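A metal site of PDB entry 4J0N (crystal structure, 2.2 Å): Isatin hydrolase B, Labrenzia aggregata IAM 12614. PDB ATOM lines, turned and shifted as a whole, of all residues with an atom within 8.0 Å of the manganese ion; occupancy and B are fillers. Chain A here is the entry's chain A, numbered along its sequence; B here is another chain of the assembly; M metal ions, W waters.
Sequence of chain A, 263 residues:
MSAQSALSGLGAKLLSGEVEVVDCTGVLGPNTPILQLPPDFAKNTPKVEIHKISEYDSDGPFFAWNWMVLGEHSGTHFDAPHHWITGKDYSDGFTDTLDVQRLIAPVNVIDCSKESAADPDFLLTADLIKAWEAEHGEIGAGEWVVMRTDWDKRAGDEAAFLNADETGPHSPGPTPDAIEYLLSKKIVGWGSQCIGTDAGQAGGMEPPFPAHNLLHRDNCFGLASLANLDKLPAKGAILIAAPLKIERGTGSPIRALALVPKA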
ATOM      1  N   LEU A  35      27.508 -27.774  29.886  1.00  0.00           N
ATOM      2  CA  LEU A  35      27.237 -28.585  28.689  1.00  0.00           C
ATOM      3  C   LEU A  35      28.320 -28.505  27.591  1.00  0.00           C
ATOM      4  O   LEU A  35      28.840 -27.422  27.291  1.00  0.00           O
ATOM      5  CB  LEU A  35      25.893 -28.180  28.081  1.00  0.00           C
ATOM      6  CG  LEU A  35      25.512 -28.787  26.732  1.00  0.00           C
ATOM      7  CD1 LEU A  35      25.177 -30.272  26.862  1.00  0.00           C
ATOM      8  CD2 LEU A  35      24.345 -27.998  26.096  1.00  0.00           C
ATOM      9  N   THR A  45      28.333 -22.906  25.001  1.00  0.00           N
ATOM     10  CA  THR A  45      28.120 -21.826  25.966  1.00  0.00           C
ATOM     11  C   THR A  45      29.358 -21.750  26.882  1.00  0.00           C
ATOM     12  O   THR A  45      29.948 -22.786  27.231  1.00  0.00           O
ATOM     13  CB  THR A  45      26.821 -22.047  26.754  1.00  0.00           C
ATOM     14  OG1 THR A  45      26.585 -20.943  27.648  1.00  0.00           O
ATOM     15  CG2 THR A  45      26.886 -23.349  27.544  1.00  0.00           C
ATOM     16  N   GLU A  72      23.629 -17.916  29.937  1.00  0.00           N
ATOM     17  CA  GLU A  72      22.260 -18.040  30.426  1.00  0.00           C
ATOM     18  C   GLU A  72      22.065 -19.437  31.025  1.00  0.00           C
ATOM     19  O   GLU A  72      21.500 -19.603  32.102  1.00  0.00           O
ATOM     20  CB  GLU A  72      21.253 -17.830  29.279  1.00  0.00           C
ATOM     21  CG  GLU A  72      21.106 -16.397  28.776  1.00  0.00           C
ATOM     22  CD  GLU A  72      20.138 -16.298  27.603  1.00  0.00           C
ATOM     23  OE1 GLU A  72      19.976 -17.317  26.884  1.00  0.00           O
ATOM     24  OE2 GLU A  72      19.540 -15.207  27.394  1.00  0.00           O
ATOM     25  N   HIS A  73      22.568 -20.427  30.300  1.00  0.00           N
ATOM     26  CA  HIS A  73      22.414 -21.826  30.708  1.00  0.00           C
ATOM     27  C   HIS A  73      23.640 -22.305  31.497  1.00  0.00           C
ATOM     28  O   HIS A  73      24.489 -23.005  30.969  1.00  0.00           O
ATOM     29  CB  HIS A  73      22.155 -22.682  29.462  1.00  0.00           C
ATOM     30  CG  HIS A  73      20.917 -22.259  28.717  1.00  0.00           C
ATOM     31  ND1 HIS A  73      19.789 -23.053  28.646  1.00  0.00           N
ATOM     32  CD2 HIS A  73      20.610 -21.116  28.070  1.00  0.00           C
ATOM     33  CE1 HIS A  73      18.852 -22.411  27.967  1.00  0.00           C
ATOM     34  NE2 HIS A  73      19.323 -21.240  27.602  1.00  0.00           N
ATOM     35  N   SER A  74      23.713 -21.930  32.766  1.00  0.00           N
ATOM     36  CA  SER A  74      24.879 -22.220  33.587  1.00  0.00           C
ATOM     37  C   SER A  74      24.471 -22.735  34.966  1.00  0.00           C
ATOM     38  O   SER A  74      23.721 -22.062  35.698  1.00  0.00           O
ATOM     39  CB  SER A  74      25.761 -20.961  33.735  1.00  0.00           C
ATOM     40  OG  SER A  74      26.102 -20.405  32.475  1.00  0.00           O
ATOM     41  N   GLY A  75      24.981 -23.906  35.335  1.00  0.00           N
ATOM     42  CA  GLY A  75      24.685 -24.487  36.643  1.00  0.00           C
ATOM     43  C   GLY A  75      23.214 -24.818  36.793  1.00  0.00           C
ATOM     44  O   GLY A  75      22.534 -25.191  35.811  1.00  0.00           O
ATOM     45  N   HIS A  77      19.782 -24.034  36.490  1.00  0.00           N
ATOM     46  CA  HIS A  77      19.228 -23.032  35.589  1.00  0.00           C
ATOM     47  C   HIS A  77      17.839 -23.363  35.002  1.00  0.00           C
ATOM     48  O   HIS A  77      17.397 -24.513  34.998  1.00  0.00           O
ATOM     49  CB  HIS A  77      20.254 -22.681  34.499  1.00  0.00           C
ATOM     50  CG  HIS A  77      20.343 -23.690  33.386  1.00  0.00           C
ATOM     51  ND1 HIS A  77      21.253 -24.737  33.404  1.00  0.00           N
ATOM     52  CD2 HIS A  77      19.655 -23.803  32.227  1.00  0.00           C
ATOM     53  CE1 HIS A  77      21.101 -25.449  32.308  1.00  0.00           C
ATOM     54  NE2 HIS A  77      20.152 -24.912  31.561  1.00  0.00           N
ATOM     55  N   PHE A  78      17.191 -22.307  34.498  1.00  0.00           N
ATOM     56  CA  PHE A  78      15.838 -22.328  33.958  1.00  0.00           C
ATOM     57  C   PHE A  78      15.876 -22.266  32.420  1.00  0.00           C
ATOM     58  O   PHE A  78      16.676 -21.513  31.868  1.00  0.00           O
ATOM     59  CB  PHE A  78      15.103 -21.089  34.526  1.00  0.00           C
ATOM     60  CG  PHE A  78      13.682 -20.916  34.059  1.00  0.00           C
ATOM     61  CD1 PHE A  78      13.394 -20.326  32.832  1.00  0.00           C
ATOM     62  CD2 PHE A  78      12.615 -21.282  34.875  1.00  0.00           C
ATOM     63  CE1 PHE A  78      12.083 -20.152  32.421  1.00  0.00           C
ATOM     64  CE2 PHE A  78      11.297 -21.098  34.470  1.00  0.00           C
ATOM     65  CZ  PHE A  78      11.031 -20.532  33.243  1.00  0.00           C
ATOM     66  N   ASP A  79      15.038 -23.060  31.756  1.00  0.00           N
ATOM     67  CA  ASP A  79      14.868 -22.999  30.294  1.00  0.00           C
ATOM     68  C   ASP A  79      13.553 -22.306  29.932  1.00  0.00           C
ATOM     69  O   ASP A  79      12.487 -22.813  30.270  1.00  0.00           O
ATOM     70  CB  ASP A  79      14.857 -24.402  29.694  1.00  0.00           C
ATOM     71  CG  ASP A  79      16.215 -25.094  29.758  1.00  0.00           C
ATOM     72  OD1 ASP A  79      17.251 -24.431  29.544  1.00  0.00           O
ATOM     73  OD2 ASP A  79      16.230 -26.324  30.017  1.00  0.00           O
ATOM     74  N   ALA A  80      13.629 -21.160  29.263  1.00  0.00           N
ATOM     75  CA  ALA A  80      12.435 -20.461  28.786  1.00  0.00           C
ATOM     76  C   ALA A  80      12.055 -21.015  27.414  1.00  0.00           C
ATOM     77  O   ALA A  80      12.917 -21.504  26.689  1.00  0.00           O
ATOM     78  CB  ALA A  80      12.692 -18.956  28.713  1.00  0.00           C
ATOM     79  N   HIS A  83      14.040 -20.902  24.056  1.00  0.00           N
ATOM     80  CA  HIS A  83      15.293 -21.631  23.952  1.00  0.00           C
ATOM     81  C   HIS A  83      15.277 -22.658  22.813  1.00  0.00           C
ATOM     82  O   HIS A  83      16.316 -22.965  22.214  1.00  0.00           O
ATOM     83  CB  HIS A  83      15.604 -22.320  25.295  1.00  0.00           C
ATOM     84  CG  HIS A  83      16.893 -23.068  25.312  1.00  0.00           C
ATOM     85  ND1 HIS A  83      18.086 -22.519  24.879  1.00  0.00           N
ATOM     86  CD2 HIS A  83      17.199 -24.334  25.701  1.00  0.00           C
ATOM     87  CE1 HIS A  83      19.056 -23.403  24.990  1.00  0.00           C
ATOM     88  NE2 HIS A  83      18.535 -24.517  25.497  1.00  0.00           N
ATOM     89  N   TRP A  84      14.108 -23.189  22.502  1.00  0.00           N
ATOM     90  CA  TRP A  84      14.000 -24.129  21.390  1.00  0.00           C
ATOM     91  C   TRP A  84      13.201 -23.563  20.216  1.00  0.00           C
ATOM     92  O   TRP A  84      12.299 -22.728  20.387  1.00  0.00           O
ATOM     93  CB  TRP A  84      13.355 -25.429  21.855  1.00  0.00           C
ATOM     94  CG  TRP A  84      14.062 -26.631  21.321  1.00  0.00           C
ATOM     95  CD1 TRP A  84      13.613 -27.504  20.349  1.00  0.00           C
ATOM     96  CD2 TRP A  84      15.367 -27.097  21.698  1.00  0.00           C
ATOM     97  NE1 TRP A  84      14.549 -28.486  20.131  1.00  0.00           N
ATOM     98  CE2 TRP A  84      15.638 -28.249  20.939  1.00  0.00           C
ATOM     99  CE3 TRP A  84      16.333 -26.642  22.609  1.00  0.00           C
ATOM    100  CZ2 TRP A  84      16.841 -28.972  21.070  1.00  0.00           C
ATOM    101  CZ3 TRP A  84      17.521 -27.350  22.747  1.00  0.00           C
ATOM    102  CH2 TRP A  84      17.757 -28.504  21.974  1.00  0.00           C
ATOM    103  N   ILE A 195      22.998 -32.200  33.449  1.00  0.00           N
ATOM    104  CA  ILE A 195      23.403 -30.949  32.786  1.00  0.00           C
ATOM    105  C   ILE A 195      22.265 -30.292  32.033  1.00  0.00           C
ATOM    106  O   ILE A 195      22.251 -29.060  31.830  1.00  0.00           O
ATOM    107  CB  ILE A 195      24.577 -31.165  31.822  1.00  0.00           C
ATOM    108  CG1 ILE A 195      25.216 -29.829  31.427  1.00  0.00           C
ATOM    109  CG2 ILE A 195      24.152 -32.003  30.614  1.00  0.00           C
ATOM    110  CD1 ILE A 195      25.959 -29.138  32.612  1.00  0.00           C
ATOM    111  N   GLY A 196      21.291 -31.103  31.634  1.00  0.00           N
ATOM    112  CA  GLY A 196      20.139 -30.631  30.893  1.00  0.00           C
ATOM    113  C   GLY A 196      18.940 -31.497  31.215  1.00  0.00           C
ATOM    114  O   GLY A 196      19.053 -32.507  31.933  1.00  0.00           O
ATOM    115  N   THR A 197      17.799 -31.101  30.674  1.00  0.00           N
ATOM    116  CA  THR A 197      16.529 -31.777  30.914  1.00  0.00           C
ATOM    117  C   THR A 197      16.416 -33.111  30.173  1.00  0.00           C
ATOM    118  O   THR A 197      15.594 -33.937  30.529  1.00  0.00           O
ATOM    119  CB  THR A 197      15.339 -30.893  30.488  1.00  0.00           C
ATOM    120  OG1 THR A 197      15.554 -30.447  29.142  1.00  0.00           O
ATOM    121  CG2 THR A 197      15.203 -29.685  31.428  1.00  0.00           C
ATOM    122  N   HIS A 212      13.450 -30.798  25.738  1.00  0.00           N
ATOM    123  CA  HIS A 212      13.588 -29.436  25.197  1.00  0.00           C
ATOM    124  C   HIS A 212      12.530 -29.194  24.114  1.00  0.00           C
ATOM    125  O   HIS A 212      11.871 -28.147  24.106  1.00  0.00           O
ATOM    126  CB  HIS A 212      14.978 -29.232  24.593  1.00  0.00           C
ATOM    127  CG  HIS A 212      16.077 -29.178  25.603  1.00  0.00           C
ATOM    128  ND1 HIS A 212      16.747 -30.307  26.038  1.00  0.00           N
ATOM    129  CD2 HIS A 212      16.626 -28.143  26.273  1.00  0.00           C
ATOM    130  CE1 HIS A 212      17.652 -29.966  26.925  1.00  0.00           C
ATOM    131  NE2 HIS A 212      17.600 -28.651  27.096  1.00  0.00           N
ATOM    132  N   HIS A 216       8.899 -26.928  25.402  1.00  0.00           N
ATOM    133  CA  HIS A 216       8.926 -25.570  24.899  1.00  0.00           C
ATOM    134  C   HIS A 216       7.920 -25.359  23.780  1.00  0.00           C
ATOM    135  O   HIS A 216       7.397 -24.246  23.605  1.00  0.00           O
ATOM    136  CB  HIS A 216      10.364 -25.210  24.501  1.00  0.00           C
ATOM    137  CG  HIS A 216      11.326 -25.323  25.647  1.00  0.00           C
ATOM    138  ND1 HIS A 216      10.995 -24.951  26.945  1.00  0.00           N
ATOM    139  CD2 HIS A 216      12.608 -25.759  25.712  1.00  0.00           C
ATOM    140  CE1 HIS A 216      12.025 -25.152  27.737  1.00  0.00           C
ATOM    141  NE2 HIS A 216      13.026 -25.647  27.017  1.00  0.00           N
ATOM    142  N   GLY A 222      11.782 -25.781  31.671  1.00  0.00           N
ATOM    143  CA  GLY A 222      12.717 -26.826  32.056  1.00  0.00           C
ATOM    144  C   GLY A 222      13.671 -26.299  33.107  1.00  0.00           C
ATOM    145  O   GLY A 222      13.958 -25.105  33.133  1.00  0.00           O
ATOM    146  N   LEU A 223      14.134 -27.185  33.992  1.00  0.00           N
ATOM    147  CA  LEU A 223      15.174 -26.860  34.968  1.00  0.00           C
ATOM    148  C   LEU A 223      16.262 -27.920  34.834  1.00  0.00           C
ATOM    149  O   LEU A 223      15.970 -29.097  34.574  1.00  0.00           O
ATOM    150  CB  LEU A 223      14.606 -26.889  36.395  1.00  0.00           C
ATOM    151  CG  LEU A 223      13.297 -26.115  36.653  1.00  0.00           C
ATOM    152  CD1 LEU A 223      12.747 -26.429  38.059  1.00  0.00           C
ATOM    153  CD2 LEU A 223      13.497 -24.613  36.461  1.00  0.00           C
ATOM    154  N   ALA A 224      17.526 -27.519  35.012  1.00  0.00           N
ATOM    155  CA  ALA A 224      18.644 -28.460  34.910  1.00  0.00           C
ATOM    156  C   ALA A 224      19.632 -28.260  36.061  1.00  0.00           C
ATOM    157  O   ALA A 224      19.678 -27.180  36.682  1.00  0.00           O
ATOM    158  CB  ALA A 224      19.331 -28.309  33.577  1.00  0.00           C
ATOM    159  N   THR A 250      16.700 -16.430  26.999  1.00  0.00           N
ATOM    160  CA  THR A 250      16.199 -17.760  26.641  1.00  0.00           C
ATOM    161  C   THR A 250      16.224 -18.707  27.847  1.00  0.00           C
ATOM    162  O   THR A 250      15.717 -19.831  27.788  1.00  0.00           O
ATOM    163  CB  THR A 250      17.070 -18.398  25.531  1.00  0.00           C
ATOM    164  OG1 THR A 250      18.259 -18.960  26.111  1.00  0.00           O
ATOM    165  CG2 THR A 250      17.468 -17.334  24.512  1.00  0.00           C
ATOM    166  N   GLY A 251      16.864 -18.253  28.927  1.00  0.00           N
ATOM    167  CA  GLY A 251      17.028 -19.053  30.119  1.00  0.00           C
ATOM    168  C   GLY A 251      17.794 -18.230  31.137  1.00  0.00           C
ATOM    169  O   GLY A 251      18.113 -17.083  30.860  1.00  0.00           O
ATOM    170  N   SER A 252      18.089 -18.803  32.300  1.00  0.00           N
ATOM    171  CA  SER A 252      18.825 -18.074  33.349  1.00  0.00           C
ATOM    172  C   SER A 252      19.321 -19.013  34.447  1.00  0.00           C
ATOM    173  O   SER A 252      18.629 -19.965  34.811  1.00  0.00           O
ATOM    174  CB  SER A 252      17.917 -16.983  33.960  1.00  0.00           C
ATOM    175  OG  SER A 252      18.420 -16.495  35.197  1.00  0.00           O
ATOM    176  N   ALA B  64      18.158 -21.324  20.700  1.00  0.00           N
ATOM    177  CA  ALA B  64      18.617 -19.960  20.867  1.00  0.00           C
ATOM    178  C   ALA B  64      19.104 -19.789  22.289  1.00  0.00           C
ATOM    179  O   ALA B  64      18.441 -20.232  23.255  1.00  0.00           O
ATOM    180  CB  ALA B  64      17.489 -18.983  20.544  1.00  0.00           C
ATOM    181  N   TRP B  65      20.276 -19.172  22.442  1.00  0.00           N
ATOM    182  CA  TRP B  65      20.827 -18.901  23.769  1.00  0.00           C
ATOM    183  C   TRP B  65      21.901 -17.825  23.734  1.00  0.00           C
ATOM    184  O   TRP B  65      22.427 -17.473  22.667  1.00  0.00           O
ATOM    185  CB  TRP B  65      21.314 -20.181  24.473  1.00  0.00           C
ATOM    186  CG  TRP B  65      22.245 -21.065  23.679  1.00  0.00           C
ATOM    187  CD1 TRP B  65      22.524 -21.001  22.342  1.00  0.00           C
ATOM    188  CD2 TRP B  65      22.998 -22.181  24.183  1.00  0.00           C
ATOM    189  NE1 TRP B  65      23.415 -21.984  21.984  1.00  0.00           N
ATOM    190  CE2 TRP B  65      23.724 -22.725  23.102  1.00  0.00           C
ATOM    191  CE3 TRP B  65      23.147 -22.764  25.448  1.00  0.00           C
ATOM    192  CZ2 TRP B  65      24.572 -23.841  23.243  1.00  0.00           C
ATOM    193  CZ3 TRP B  65      23.992 -23.864  25.589  1.00  0.00           C
ATOM    194  CH2 TRP B  65      24.696 -24.383  24.493  1.00  0.00           C
HETATM  195 MN    MN M   1      19.416 -24.990  29.483  1.00  0.00          MN
HETATM  196  O   HOH W   1      18.332 -27.738  30.072  1.00  0.00           O
HETATM  197  O   HOH W   2      20.293 -26.110  27.876  1.00  0.00           O
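A ring nitrogen (ND1) of His 73 is bound to the manganese ion (2.1 Å).
Water W2 binds the manganese ion.
The manganese ion is bound by NE2 of His 77 (2.2 Å).
The manganese ion is bound by the side-chain carboxylate (OD1) of Asp 79 (2.2 Å).
Water W1 lies within hydrogen-bond range of OD2 of Asp 79 (2.5 Å), NE2 of His 212 (3.2 Å) and N of Thr 197 (3.5 Å).
The side-chain hydroxyl (OG1) of Thr 250 sits at hydrogen-bond distance from a ring nitrogen (NE2) of His 73 (2.9 Å).
A ring nitrogen (NE2) of His 73 sits close to a ring nitrogen (ND1) of His 83, at 3.3 Å.
N of Ala 224 sits at hydrogen-bond distance from O of His 77, 3.0 Å away.
N of Asp 79 sits at hydrogen-bond distance from O of Gly 222 (2.7 Å).
The backbone carbonyl oxygen (O) of Gly 75 lies within hydrogen-bond range of a ring nitrogen (ND1) of His 77, at 2.8 Å.
Of the 25 residues printed, 3 come within 4 Å of the manganese ion.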
